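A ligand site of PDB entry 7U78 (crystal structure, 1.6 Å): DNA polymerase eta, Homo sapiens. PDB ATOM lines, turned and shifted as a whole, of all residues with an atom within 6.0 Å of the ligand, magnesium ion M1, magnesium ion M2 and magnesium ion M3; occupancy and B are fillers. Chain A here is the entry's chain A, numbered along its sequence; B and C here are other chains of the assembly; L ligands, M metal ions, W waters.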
ATOM      1  N   ASP A  16     -12.980  30.784 -14.100  1.00  0.00           N
ATOM      2  CA  ASP A  16     -13.735  30.195 -12.980  1.00  0.00           C
ATOM      3  C   ASP A  16     -13.741  31.176 -11.811  1.00  0.00           C
ATOM      4  O   ASP A  16     -12.666  31.676 -11.422  1.00  0.00           O
ATOM      5  CB  ASP A  16     -13.109  28.862 -12.660  1.00  0.00           C
ATOM      6  CG  ASP A  16     -13.666  28.227 -11.418  1.00  0.00           C
ATOM      7  OD1 ASP A  16     -14.737  28.625 -10.934  1.00  0.00           O
ATOM      8  OD2 ASP A  16     -13.019  27.273 -11.010  1.00  0.00           O
ATOM      9  N   MET A  17     -14.925  31.385 -11.238  1.00  0.00           N
ATOM     10  CA  MET A  17     -15.067  32.281 -10.067  1.00  0.00           C
ATOM     11  C   MET A  17     -14.442  31.635  -8.823  1.00  0.00           C
ATOM     12  O   MET A  17     -14.748  30.512  -8.509  1.00  0.00           O
ATOM     13  CB  MET A  17     -16.542  32.591  -9.773  1.00  0.00           C
ATOM     14  CG  MET A  17     -17.327  32.991 -10.994  1.00  0.00           C
ATOM     15  SD  MET A  17     -16.584  34.406 -11.803  1.00  0.00           S
ATOM     16  CE  MET A  17     -16.674  35.606 -10.479  1.00  0.00           C
ATOM     17  N   ASP A  18     -13.688  32.407  -8.074  1.00  0.00           N
ATOM     18  CA  ASP A  18     -13.047  31.877  -6.847  1.00  0.00           C
ATOM     19  C   ASP A  18     -14.114  31.581  -5.790  1.00  0.00           C
ATOM     20  O   ASP A  18     -14.977  32.419  -5.629  1.00  0.00           O
ATOM     21  CB  ASP A  18     -11.993  32.844  -6.327  1.00  0.00           C
ATOM     22  CG  ASP A  18     -10.888  33.151  -7.316  1.00  0.00           C
ATOM     23  OD1 ASP A  18     -10.504  32.259  -8.061  1.00  0.00           O
ATOM     24  OD2 ASP A  18     -10.413  34.286  -7.317  1.00  0.00           O
ATOM     25  N   CYS A  19     -14.008  30.436  -5.111  1.00  0.00           N
ATOM     26  CA  CYS A  19     -14.972  30.000  -4.046  1.00  0.00           C
ATOM     27  C   CYS A  19     -16.313  30.713  -4.259  1.00  0.00           C
ATOM     28  O   CYS A  19     -16.736  31.433  -3.369  1.00  0.00           O
ATOM     29  CB  CYS A  19     -14.368  30.211  -2.670  1.00  0.00           C
ATOM     30  SG  CYS A  19     -13.656  31.845  -2.380  1.00  0.00           S
ATOM     31  N   PHE A  20     -16.967  30.421  -5.378  1.00  0.00           N
ATOM     32  CA  PHE A  20     -18.133  31.226  -5.807  1.00  0.00           C
ATOM     33  C   PHE A  20     -19.198  31.446  -4.723  1.00  0.00           C
ATOM     34  O   PHE A  20     -19.477  32.591  -4.432  1.00  0.00           O
ATOM     35  CB  PHE A  20     -18.757  30.629  -7.076  1.00  0.00           C
ATOM     36  CG  PHE A  20     -19.795  31.516  -7.702  1.00  0.00           C
ATOM     37  CD1 PHE A  20     -19.561  32.872  -7.864  1.00  0.00           C
ATOM     38  CD2 PHE A  20     -21.005  31.007  -8.111  1.00  0.00           C
ATOM     39  CE1 PHE A  20     -20.510  33.695  -8.439  1.00  0.00           C
ATOM     40  CE2 PHE A  20     -21.966  31.829  -8.677  1.00  0.00           C
ATOM     41  CZ  PHE A  20     -21.705  33.171  -8.853  1.00  0.00           C
ATOM     42  N   PHE A  21     -19.799  30.382  -4.224  1.00  0.00           N
ATOM     43  CA  PHE A  21     -20.910  30.615  -3.299  1.00  0.00           C
ATOM     44  C   PHE A  21     -20.439  31.399  -2.074  1.00  0.00           C
ATOM     45  O   PHE A  21     -21.203  32.208  -1.523  1.00  0.00           O
ATOM     46  CB  PHE A  21     -21.559  29.300  -2.841  1.00  0.00           C
ATOM     47  CG  PHE A  21     -22.377  28.578  -3.879  1.00  0.00           C
ATOM     48  CD1 PHE A  21     -22.263  28.853  -5.247  1.00  0.00           C
ATOM     49  CD2 PHE A  21     -23.232  27.564  -3.469  1.00  0.00           C
ATOM     50  CE1 PHE A  21     -23.007  28.137  -6.167  1.00  0.00           C
ATOM     51  CE2 PHE A  21     -23.987  26.857  -4.390  1.00  0.00           C
ATOM     52  CZ  PHE A  21     -23.859  27.148  -5.749  1.00  0.00           C
ATOM     53  N   VAL A  22     -19.197  31.165  -1.627  1.00  0.00           N
ATOM     54  CA  VAL A  22     -18.642  31.975  -0.549  1.00  0.00           C
ATOM     55  C   VAL A  22     -18.620  33.445  -0.938  1.00  0.00           C
ATOM     56  O   VAL A  22     -18.992  34.323  -0.155  1.00  0.00           O
ATOM     57  CB  VAL A  22     -17.240  31.479  -0.173  1.00  0.00           C
ATOM     58  CG1 VAL A  22     -16.521  32.524   0.690  1.00  0.00           C
ATOM     59  CG2 VAL A  22     -17.361  30.163   0.596  1.00  0.00           C
ATOM     60  N   GLN A  41     -24.977  23.382   3.338  1.00  0.00           N
ATOM     61  CA  GLN A  41     -26.370  23.039   3.072  1.00  0.00           C
ATOM     62  C   GLN A  41     -26.907  22.268   4.268  1.00  0.00           C
ATOM     63  O   GLN A  41     -26.311  21.263   4.668  1.00  0.00           O
ATOM     64  CB  GLN A  41     -26.518  22.192   1.799  1.00  0.00           C
ATOM     65  CG  GLN A  41     -26.021  22.873   0.530  1.00  0.00           C
ATOM     66  CD  GLN A  41     -26.337  22.082  -0.724  1.00  0.00           C
ATOM     67  OE1 GLN A  41     -27.009  22.583  -1.633  1.00  0.00           O
ATOM     68  NE2 GLN A  41     -25.833  20.846  -0.815  1.00  0.00           N
ATOM     69  N   ILE A  51     -20.146  23.035   1.017  1.00  0.00           N
ATOM     70  CA  ILE A  51     -20.043  22.974  -0.442  1.00  0.00           C
ATOM     71  C   ILE A  51     -19.132  24.030  -1.037  1.00  0.00           C
ATOM     72  O   ILE A  51     -18.813  23.944  -2.222  1.00  0.00           O
ATOM     73  CB  ILE A  51     -21.439  23.015  -1.117  1.00  0.00           C
ATOM     74  CG1 ILE A  51     -22.221  24.251  -0.694  1.00  0.00           C
ATOM     75  CG2 ILE A  51     -22.219  21.732  -0.824  1.00  0.00           C
ATOM     76  CD1 ILE A  51     -23.506  24.426  -1.531  1.00  0.00           C
ATOM     77  N   ALA A  52     -18.650  24.991  -0.252  1.00  0.00           N
ATOM     78  CA  ALA A  52     -17.729  26.004  -0.766  1.00  0.00           C
ATOM     79  C   ALA A  52     -16.938  26.565   0.399  1.00  0.00           C
ATOM     80  O   ALA A  52     -17.458  26.655   1.500  1.00  0.00           O
ATOM     81  CB  ALA A  52     -18.479  27.159  -1.477  1.00  0.00           C
ATOM     82  N   VAL A  53     -15.673  26.930   0.147  1.00  0.00           N
ATOM     83  CA  VAL A  53     -14.712  27.239   1.210  1.00  0.00           C
ATOM     84  C   VAL A  53     -13.826  28.401   0.797  1.00  0.00           C
ATOM     85  O   VAL A  53     -13.197  28.347  -0.267  1.00  0.00           O
ATOM     86  CB  VAL A  53     -13.842  26.023   1.550  1.00  0.00           C
ATOM     87  CG1 VAL A  53     -12.894  26.339   2.705  1.00  0.00           C
ATOM     88  CG2 VAL A  53     -14.693  24.827   1.895  1.00  0.00           C
ATOM     89  N   TYR A  55     -10.549  30.823   0.716  1.00  0.00           N
ATOM     90  CA  TYR A  55      -9.134  30.428   0.738  1.00  0.00           C
ATOM     91  C   TYR A  55      -8.515  30.549   2.131  1.00  0.00           C
ATOM     92  O   TYR A  55      -7.660  29.719   2.511  1.00  0.00           O
ATOM     93  CB  TYR A  55      -8.375  31.230  -0.324  1.00  0.00           C
ATOM     94  CG  TYR A  55      -8.648  30.640  -1.700  1.00  0.00           C
ATOM     95  CD1 TYR A  55      -9.853  30.858  -2.356  1.00  0.00           C
ATOM     96  CD2 TYR A  55      -7.727  29.789  -2.310  1.00  0.00           C
ATOM     97  CE1 TYR A  55     -10.132  30.278  -3.604  1.00  0.00           C
ATOM     98  CE2 TYR A  55      -7.988  29.221  -3.554  1.00  0.00           C
ATOM     99  CZ  TYR A  55      -9.191  29.455  -4.192  1.00  0.00           C
ATOM    100  OH  TYR A  55      -9.445  28.884  -5.428  1.00  0.00           O
ATOM    101  N   ARG A  58      -9.459  27.352   3.670  1.00  0.00           N
ATOM    102  CA  ARG A  58      -8.730  26.240   3.072  1.00  0.00           C
ATOM    103  C   ARG A  58      -7.353  26.071   3.709  1.00  0.00           C
ATOM    104  O   ARG A  58      -6.854  24.943   3.814  1.00  0.00           O
ATOM    105  CB  ARG A  58      -8.593  26.446   1.565  1.00  0.00           C
ATOM    106  CG  ARG A  58      -9.895  26.467   0.809  1.00  0.00           C
ATOM    107  CD  ARG A  58      -9.657  26.678  -0.655  1.00  0.00           C
ATOM    108  NE  ARG A  58     -10.916  26.903  -1.360  1.00  0.00           N
ATOM    109  CZ  ARG A  58     -11.074  26.781  -2.670  1.00  0.00           C
ATOM    110  NH1 ARG A  58     -10.064  26.468  -3.457  1.00  0.00           N
ATOM    111  NH2 ARG A  58     -12.275  26.997  -3.210  1.00  0.00           N
ATOM    112  N   ARG A  64     -14.569  21.098   0.664  1.00  0.00           N
ATOM    113  CA  ARG A  64     -15.941  20.729   0.265  1.00  0.00           C
ATOM    114  C   ARG A  64     -16.168  19.274   0.699  1.00  0.00           C
ATOM    115  O   ARG A  64     -15.182  18.533   0.815  1.00  0.00           O
ATOM    116  CB  ARG A  64     -16.022  20.961  -1.250  1.00  0.00           C
ATOM    117  CG  ARG A  64     -17.325  20.559  -1.928  1.00  0.00           C
ATOM    118  CD  ARG A  64     -16.988  20.259  -3.375  1.00  0.00           C
ATOM    119  NE  ARG A  64     -18.053  19.432  -3.908  1.00  0.00           N
ATOM    120  CZ  ARG A  64     -17.966  18.122  -4.120  1.00  0.00           C
ATOM    121  NH1 ARG A  64     -16.837  17.483  -3.859  1.00  0.00           N
ATOM    122  NH2 ARG A  64     -19.013  17.458  -4.586  1.00  0.00           N
ATOM    123  N   SER A  65     -17.435  18.906   0.937  1.00  0.00           N
ATOM    124  CA  SER A  65     -17.820  17.521   1.323  1.00  0.00           C
ATOM    125  C   SER A  65     -17.429  17.220   2.770  1.00  0.00           C
ATOM    126  O   SER A  65     -17.520  16.066   3.158  1.00  0.00           O
ATOM    127  CB  SER A  65     -17.306  16.481   0.376  1.00  0.00           C
ATOM    128  OG  SER A  65     -17.628  16.800  -0.970  1.00  0.00           O
ATOM    129  N   LEU A  92     -31.030  27.103  -4.527  1.00  0.00           N
ATOM    130  CA  LEU A  92     -29.792  27.742  -4.962  1.00  0.00           C
ATOM    131  C   LEU A  92     -30.021  28.954  -5.850  1.00  0.00           C
ATOM    132  O   LEU A  92     -29.113  29.357  -6.594  1.00  0.00           O
ATOM    133  CB  LEU A  92     -28.890  26.733  -5.676  1.00  0.00           C
ATOM    134  CG  LEU A  92     -28.678  25.440  -4.901  1.00  0.00           C
ATOM    135  CD1 LEU A  92     -27.967  24.436  -5.772  1.00  0.00           C
ATOM    136  CD2 LEU A  92     -27.870  25.714  -3.643  1.00  0.00           C
ATOM    137  N   SER A 116     -20.376  25.563 -16.060  1.00  0.00           N
ATOM    138  CA  SER A 116     -20.991  25.291 -14.744  1.00  0.00           C
ATOM    139  C   SER A 116     -21.589  26.595 -14.221  1.00  0.00           C
ATOM    140  O   SER A 116     -21.481  27.600 -14.883  1.00  0.00           O
ATOM    141  CB  SER A 116     -19.973  24.738 -13.764  1.00  0.00           C
ATOM    142  OG  SER A 116     -19.135  25.757 -13.242  1.00  0.00           O
ATOM    143  N   ILE A 117     -22.143  26.525 -13.013  1.00  0.00           N
ATOM    144  CA  ILE A 117     -22.709  27.749 -12.375  1.00  0.00           C
ATOM    145  C   ILE A 117     -21.636  28.831 -12.247  1.00  0.00           C
ATOM    146  O   ILE A 117     -21.980  29.990 -12.179  1.00  0.00           O
ATOM    147  CB  ILE A 117     -23.310  27.402 -10.994  1.00  0.00           C
ATOM    148  CG1 ILE A 117     -24.279  28.478 -10.506  1.00  0.00           C
ATOM    149  CG2 ILE A 117     -22.232  27.106  -9.954  1.00  0.00           C
ATOM    150  CD1 ILE A 117     -25.211  28.004  -9.428  1.00  0.00           C
ATOM    151  N   ASP A 118     -20.365  28.452 -12.227  1.00  0.00           N
ATOM    152  CA  ASP A 118     -19.391  29.526 -11.933  1.00  0.00           C
ATOM    153  C   ASP A 118     -18.221  29.516 -12.891  1.00  0.00           C
ATOM    154  O   ASP A 118     -17.192  30.113 -12.598  1.00  0.00           O
ATOM    155  CB  ASP A 118     -18.940  29.430 -10.487  1.00  0.00           C
ATOM    156  CG  ASP A 118     -17.766  28.501 -10.315  1.00  0.00           C
ATOM    157  OD1 ASP A 118     -17.789  27.399 -10.887  1.00  0.00           O
ATOM    158  OD2 ASP A 118     -16.866  28.929  -9.634  1.00  0.00           O
ATOM    159  N   GLU A 119     -18.377  28.926 -14.079  1.00  0.00           N
ATOM    160  CA  GLU A 119     -17.249  28.935 -14.995  1.00  0.00           C
ATOM    161  C   GLU A 119     -17.740  28.843 -16.423  1.00  0.00           C
ATOM    162  O   GLU A 119     -18.741  28.165 -16.730  1.00  0.00           O
ATOM    163  CB  GLU A 119     -16.257  27.804 -14.701  1.00  0.00           C
ATOM    164  CG  GLU A 119     -16.591  26.510 -15.340  1.00  0.00           C
ATOM    165  CD  GLU A 119     -15.923  25.354 -14.646  1.00  0.00           C
ATOM    166  OE1 GLU A 119     -16.064  25.274 -13.402  1.00  0.00           O
ATOM    167  OE2 GLU A 119     -15.356  24.478 -15.340  1.00  0.00           O
ATOM    168  N   LYS A 234      -4.480  29.886  -8.395  1.00  0.00           N
ATOM    169  CA  LYS A 234      -5.678  30.408  -7.748  1.00  0.00           C
ATOM    170  C   LYS A 234      -5.306  30.866  -6.343  1.00  0.00           C
ATOM    171  O   LYS A 234      -4.375  30.337  -5.725  1.00  0.00           O
ATOM    172  CB  LYS A 234      -6.799  29.352  -7.669  1.00  0.00           C
ATOM    173  CG  LYS A 234      -7.489  29.020  -9.016  1.00  0.00           C
ATOM    174  CD  LYS A 234      -8.886  28.313  -8.818  1.00  0.00           C
ATOM    175  CE  LYS A 234     -10.056  28.827  -9.724  1.00  0.00           C
ATOM    176  NZ  LYS A 234     -11.043  29.858  -9.161  1.00  0.00           N
ATOM    177  N   PRO A 235      -6.006  31.873  -5.799  1.00  0.00           N
ATOM    178  CA  PRO A 235      -7.130  32.621  -6.363  1.00  0.00           C
ATOM    179  C   PRO A 235      -6.726  33.947  -7.027  1.00  0.00           C
ATOM    180  O   PRO A 235      -5.575  34.408  -6.858  1.00  0.00           O
ATOM    181  CB  PRO A 235      -7.975  32.906  -5.117  1.00  0.00           C
ATOM    182  CG  PRO A 235      -6.927  33.153  -4.054  1.00  0.00           C
ATOM    183  CD  PRO A 235      -5.777  32.215  -4.385  1.00  0.00           C
ATOM    184  P    DT B   3     -22.045   9.736   4.266  1.00  0.00           P
ATOM    185  OP1  DT B   3     -22.202   8.409   3.624  1.00  0.00           O
ATOM    186  OP2  DT B   3     -20.758  10.091   4.911  1.00  0.00           O
ATOM    187  O5'  DT B   3     -22.363  10.874   3.203  1.00  0.00           O
ATOM    188  C5'  DT B   3     -21.660  12.131   3.237  1.00  0.00           C
ATOM    189  C4'  DT B   3     -22.453  13.232   2.591  1.00  0.00           C
ATOM    190  O4'  DT B   3     -21.538  14.036   1.809  1.00  0.00           O
ATOM    191  C3'  DT B   3     -23.535  12.780   1.615  1.00  0.00           C
ATOM    192  O3'  DT B   3     -24.552  13.775   1.443  1.00  0.00           O
ATOM    193  C2'  DT B   3     -22.737  12.633   0.329  1.00  0.00           C
ATOM    194  C1'  DT B   3     -21.778  13.818   0.428  1.00  0.00           C
ATOM    195  N1   DT B   3     -20.474  13.630  -0.242  1.00  0.00           N
ATOM    196  C2   DT B   3     -19.957  14.683  -0.973  1.00  0.00           C
ATOM    197  O2   DT B   3     -20.517  15.763  -1.050  1.00  0.00           O
ATOM    198  N3   DT B   3     -18.756  14.424  -1.579  1.00  0.00           N
ATOM    199  C4   DT B   3     -18.026  13.255  -1.537  1.00  0.00           C
ATOM    200  O4   DT B   3     -16.965  13.172  -2.135  1.00  0.00           O
ATOM    201  C5   DT B   3     -18.636  12.184  -0.768  1.00  0.00           C
ATOM    202  C7   DT B   3     -17.930  10.859  -0.679  1.00  0.00           C
ATOM    203  C6   DT B   3     -19.816  12.422  -0.173  1.00  0.00           C
ATOM    204  P    DT B   4     -26.097  13.376   1.615  1.00  0.00           P
ATOM    205  OP1  DT B   4     -26.328  13.057   3.043  1.00  0.00           O
ATOM    206  OP2  DT B   4     -26.447  12.383   0.570  1.00  0.00           O
ATOM    207  O5'  DT B   4     -26.864  14.741   1.312  1.00  0.00           O
ATOM    208  C5'  DT B   4     -26.295  16.003   1.663  1.00  0.00           C
ATOM    209  C4'  DT B   4     -26.686  17.025   0.634  1.00  0.00           C
ATOM    210  O4'  DT B   4     -25.533  17.334  -0.178  1.00  0.00           O
ATOM    211  C3'  DT B   4     -27.789  16.580  -0.335  1.00  0.00           C
ATOM    212  O3'  DT B   4     -28.687  17.677  -0.491  1.00  0.00           O
ATOM    213  C2'  DT B   4     -27.014  16.242  -1.603  1.00  0.00           C
ATOM    214  C1'  DT B   4     -25.867  17.217  -1.537  1.00  0.00           C
ATOM    215  N1   DT B   4     -24.664  16.769  -2.250  1.00  0.00           N
ATOM    216  C2   DT B   4     -23.897  17.728  -2.868  1.00  0.00           C
ATOM    217  O2   DT B   4     -24.175  18.916  -2.838  1.00  0.00           O
ATOM    218  N3   DT B   4     -22.793  17.246  -3.518  1.00  0.00           N
ATOM    219  C4   DT B   4     -22.383  15.930  -3.609  1.00  0.00           C
ATOM    220  O4   DT B   4     -21.364  15.650  -4.231  1.00  0.00           O
ATOM    221  C5   DT B   4     -23.240  14.980  -2.945  1.00  0.00           C
ATOM    222  C7   DT B   4     -22.870  13.524  -2.984  1.00  0.00           C
ATOM    223  C6   DT B   4     -24.317  15.438  -2.298  1.00  0.00           C
ATOM    224  P    DA B   5     -29.839  17.567  -1.416  1.00  0.00           P
ATOM    225  OP1  DA B   5     -31.081  18.077  -0.807  1.00  0.00           O
ATOM    226  OP2  DA B   5     -29.782  16.174  -1.906  1.00  0.00           O
ATOM    227  O5'  DA B   5     -29.486  18.500  -2.656  1.00  0.00           O
ATOM    228  C5'  DA B   5     -29.218  19.898  -2.481  1.00  0.00           C
ATOM    229  C4'  DA B   5     -28.910  20.565  -3.809  1.00  0.00           C
ATOM    230  O4'  DA B   5     -27.631  20.097  -4.285  1.00  0.00           O
ATOM    231  C3'  DA B   5     -29.918  20.281  -4.932  1.00  0.00           C
ATOM    232  O3'  DA B   5     -30.166  21.479  -5.678  1.00  0.00           O
ATOM    233  C2'  DA B   5     -29.213  19.260  -5.791  1.00  0.00           C
ATOM    234  C1'  DA B   5     -27.744  19.584  -5.606  1.00  0.00           C
ATOM    235  N9   DA B   5     -26.867  18.427  -5.711  1.00  0.00           N
ATOM    236  C8   DA B   5     -27.102  17.149  -5.290  1.00  0.00           C
ATOM    237  N7   DA B   5     -26.113  16.320  -5.518  1.00  0.00           N
ATOM    238  C5   DA B   5     -25.152  17.114  -6.127  1.00  0.00           C
ATOM    239  C6   DA B   5     -23.862  16.832  -6.626  1.00  0.00           C
ATOM    240  N6   DA B   5     -23.299  15.619  -6.580  1.00  0.00           N
ATOM    241  N1   DA B   5     -23.169  17.844  -7.178  1.00  0.00           N
ATOM    242  C2   DA B   5     -23.738  19.060  -7.232  1.00  0.00           C
ATOM    243  N3   DA B   5     -24.935  19.445  -6.802  1.00  0.00           N
ATOM    244  C4   DA B   5     -25.601  18.410  -6.254  1.00  0.00           C
ATOM    245  P    DT C   8     -13.975  19.733 -11.424  1.00  0.00           P
ATOM    246  OP1  DT C   8     -13.464  20.987 -12.014  1.00  0.00           O
ATOM    247  OP2  DT C   8     -13.026  18.694 -10.965  1.00  0.00           O
ATOM    248  O5'  DT C   8     -14.899  20.098 -10.189  1.00  0.00           O
ATOM    249  C5'  DT C   8     -16.119  20.851 -10.360  1.00  0.00           C
ATOM    250  C4'  DT C   8     -16.905  20.868  -9.070  1.00  0.00           C
ATOM    251  O4'  DT C   8     -17.901  19.819  -9.072  1.00  0.00           O
ATOM    252  C3'  DT C   8     -16.050  20.634  -7.806  1.00  0.00           C
ATOM    253  O3'  DT C   8     -16.353  21.612  -6.809  1.00  0.00           O
ATOM    254  C2'  DT C   8     -16.525  19.293  -7.280  1.00  0.00           C
ATOM    255  C1'  DT C   8     -17.962  19.314  -7.746  1.00  0.00           C
ATOM    256  N1   DT C   8     -18.588  17.994  -7.772  1.00  0.00           N
ATOM    257  C2   DT C   8     -19.958  17.959  -7.848  1.00  0.00           C
ATOM    258  O2   DT C   8     -20.643  18.960  -7.982  1.00  0.00           O
ATOM    259  N3   DT C   8     -20.501  16.694  -7.796  1.00  0.00           N
ATOM    260  C4   DT C   8     -19.827  15.505  -7.652  1.00  0.00           C
ATOM    261  O4   DT C   8     -20.446  14.445  -7.629  1.00  0.00           O
ATOM    262  C5   DT C   8     -18.391  15.622  -7.553  1.00  0.00           C
ATOM    263  C7   DT C   8     -17.565  14.384  -7.401  1.00  0.00           C
ATOM    264  C6   DT C   8     -17.846  16.846  -7.597  1.00  0.00           C
HETATM  265  P1  LIG L   1     -12.581  27.417  -6.585  1.00  0.00           P
HETATM  266  O1  LIG L   1     -11.652  26.217  -6.244  1.00  0.00           O
HETATM  267  O2  LIG L   1     -11.913  28.727  -6.184  1.00  0.00           O
HETATM  268  O3  LIG L   1     -13.140  27.400  -7.996  1.00  0.00           O
HETATM  269  O4  LIG L   1     -13.804  27.283  -5.581  1.00  0.00           O
HETATM  270  P2  LIG L   1     -15.328  27.159  -6.013  1.00  0.00           P
HETATM  271  O5  LIG L   1     -16.150  27.035  -4.715  1.00  0.00           O
HETATM  272  O6  LIG L   1     -15.784  28.209  -6.993  1.00  0.00           O
HETATM  273  O7  LIG L   1     -15.334  25.713  -6.662  1.00  0.00           O
HETATM  274  P3  LIG L   1     -15.997  25.149  -7.993  1.00  0.00           P
HETATM  275  O8  LIG L   1     -15.681  26.140  -9.126  1.00  0.00           O
HETATM  276  O9  LIG L   1     -15.533  23.732  -8.247  1.00  0.00           O
HETATM  277  O10 LIG L   1     -17.570  25.218  -7.710  1.00  0.00           O
HETATM  278  C1  LIG L   1     -18.364  26.396  -7.939  1.00  0.00           C
HETATM  279  C2  LIG L   1     -19.534  26.417  -6.990  1.00  0.00           C
HETATM  280  O11 LIG L   1     -20.346  25.238  -7.199  1.00  0.00           O
HETATM  281  C3  LIG L   1     -19.171  26.353  -5.502  1.00  0.00           C
HETATM  282  O12 LIG L   1     -18.917  27.641  -4.951  1.00  0.00           O
HETATM  283  C4  LIG L   1     -20.458  25.812  -4.896  1.00  0.00           C
HETATM  284  C5  LIG L   1     -21.011  24.902  -5.990  1.00  0.00           C
HETATM  285  N1  LIG L   1     -20.800  23.485  -5.718  1.00  0.00           N
HETATM  286  C6  LIG L   1     -19.645  22.764  -5.803  1.00  0.00           C
HETATM  287  N2  LIG L   1     -19.816  21.494  -5.402  1.00  0.00           N
HETATM  288  C7  LIG L   1     -21.155  21.429  -5.062  1.00  0.00           C
HETATM  289  C8  LIG L   1     -21.965  20.371  -4.559  1.00  0.00           C
HETATM  290  O13 LIG L   1     -21.509  19.240  -4.343  1.00  0.00           O
HETATM  291  N3  LIG L   1     -23.263  20.600  -4.302  1.00  0.00           N
HETATM  292  C9  LIG L   1     -23.747  21.881  -4.554  1.00  0.00           C
HETATM  293  N4  LIG L   1     -25.044  22.056  -4.293  1.00  0.00           N
HETATM  294  N5  LIG L   1     -23.043  22.906  -5.015  1.00  0.00           N
HETATM  295  C10 LIG L   1     -21.755  22.625  -5.247  1.00  0.00           C
HETATM  296 MG    MG M   1     -16.175  26.040 -11.404  1.00  0.00          MG
HETATM  297 MG    MG M   2     -14.841  28.295  -8.998  1.00  0.00          MG
HETATM  298 MG    MG M   3     -13.905  23.767  -6.351  1.00  0.00          MG
HETATM  299  O   HOH W   1     -16.585  24.051  -3.905  1.00  0.00           O
HETATM  300  O   HOH W   2     -17.462  24.168 -10.806  1.00  0.00           O
HETATM  301  O   HOH W   3     -12.802  24.967  -9.000  1.00  0.00           O
HETATM  302  O   HOH W   4     -13.814  23.762  -2.917  1.00  0.00           O
HETATM  303  O   HOH W   5     -12.232  24.211  -5.355  1.00  0.00           O
HETATM  304  O   HOH W   6     -12.561  22.565  -7.498  1.00  0.00           O
HETATM  305  O   HOH W   7     -14.785  26.163  -2.514  1.00  0.00           O
HETATM  306  O   HOH W   8     -14.398  24.395 -10.891  1.00  0.00           O
HETATM  307  O   HOH W   9     -15.030  22.854  -5.332  1.00  0.00           O
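Merely in contact with magnesium ion M3: DT 8 of chain C. Of the 26 residues printed, 1 comes within 4 Å of magnesium ion M3. The nearest printed residue that does not touch magnesium ion M3 is Arg 58 (4.8 Å).
Water W2 bridges O10 of the ligand and OG of Ser 116. Water W3 bridges OD2 of Asp 16 and O1 of the ligand. Water W7 lies within hydrogen-bond range of an oxygen (O5) of the ligand (2.7 Å), the guanidinium group of Arg 58 (2.7 Å) and the backbone NH of Val 53 (2.9 Å). Water W1 lies within hydrogen-bond range of O of Ile 51 and O5 of the ligand.
Magnesium ion M1 is bound by the side-chain carboxylate of Glu 119 (2.1 Å), the side-chain carboxylate of Asp 118 (2.2 Å), an oxygen (O8) of the ligand (2.3 Å), water W2 (2.3 Å) and water W8 (2.5 Å). Magnesium ion M1 has five donor atoms within binding distance.
O2 of DT 4 of chain B sits at hydrogen-bond distance from NE2 of Gln 41, at 3.3 Å. The backbone NH (N) of Glu 119 is in hydrogen-bond range of the side-chain hydroxyl (OG) of Ser 116 (3.4 Å). The side-chain carboxylate (OD2) of Asp 16 is in salt-bridge range of the side-chain amino group (NZ) of Lys 234 (3.7 Å). OH of Tyr 55 is in hydrogen-bond range of NH1 of Arg 58 (3.2 Å). The side-chain carboxylate (OD1) of Asp 18 is in salt-bridge range of the side-chain amino group (NZ) of Lys 234, at 2.7 Å. OG of Ser 116 sits close to N of Asp 118, at 3.1 Å. The guanidinium group of Arg 58 is in hydrogen-bond range of the backbone carbonyl oxygen of Val 53 (2.9 Å). O4 of DT 4 of chain B sits at hydrogen-bond distance from NH2 of Arg 64.
Magnesium ion M2 is bound by the side-chain carboxylate (OD1) of Asp 16, an oxygen (O3) of the ligand, the side-chain carboxylate (OD2) of Asp 118, an oxygen (O6) of the ligand, the backbone carbonyl oxygen (O) of Met 17 and an oxygen (O8) of the ligand.
Magnesium ion M3 is bound by water W9 (1.8 Å). Water W5 is bound to magnesium ion M3, 2.0 Å away. Water W6 is bound to magnesium ion M3 (2.1 Å). Magnesium ion M3 is bound by O7 of the ligand, at 2.4 Å. O9 of the ligand binds magnesium ion M3 (2.5 Å).
The side-chain amino group (NZ) of Lys 234 is in salt-bridge range of an oxygen (O2) of the ligand, at 3.3 Å. N of Phe 20 sits at hydrogen-bond distance from O12 of the ligand (3.4 Å). An oxygen (O1) of the ligand lies within salt-bridge range of the guanidinium group (NH2) of Arg 58 (3.2 Å). N of Cys 19 lies within hydrogen-bond range of O2 of the ligand. O3' of DT 8 of chain C lies close to O9 of the ligand (2.7 Å). A nitrogen (N3) of the ligand is in hydrogen-bond range of O2 of DT 4 of chain B, at 2.4 Å. An oxygen (O12) of the ligand is in hydrogen-bond range of the backbone NH (N) of Phe 21 (3.0 Å). O4' of DA 5 of chain B lies within hydrogen-bond range of N4 of the ligand (3.2 Å). O2 of the ligand sits at hydrogen-bond distance from OH of Tyr 55, 2.6 Å away. The side-chain amide oxygen of Gln 41 lies within hydrogen-bond range of a nitrogen (N4) of the ligand (3.3 Å). N3 of DA 5 of chain B lies within hydrogen-bond range of N3 of the ligand, 3.2 Å away. O13 of the ligand is in hydrogen-bond range of NH2 of Arg 64 (3.1 Å).
Residues that only touch magnesium ion M1: Ser 116 (3.5 Å). Within 4 Å of magnesium ion M1: Asp 16, Ser 116, Asp 118 and Glu 119. The nearest printed residue that does not touch magnesium ion M1 is DT 8 of chain C (5.3 Å).
The nearest printed residue that does not touch magnesium ion M2 is Lys 234 (4.1 Å).
CA of Asp 18 touches O2 of the ligand, 3.4 Å away. Ile 51 touches the ligand (O to C4, 3.7 Å). Ala 52 touches the ligand (CB to O12, 3.5 Å). CG2 of Ile 117 touches O11 of the ligand, at 3.8 Å. Hydrophobic or aromatic side chains that line the ligand: Phe 20, Phe 21, Ile 51, Ala 52, Tyr 55 and Ile 117. 18 residues have an atom within 4 Å of the ligand: Asp 16, Met 17, Asp 18, Cys 19, Phe 20, Phe 21, Gln 41, Ile 51, Ala 52, Tyr 55, Arg 58, Arg 64, Ile 117, Asp 118, Lys 234, DT 4 of chain B, DA 5 of chain B and DT 8 of chain C.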
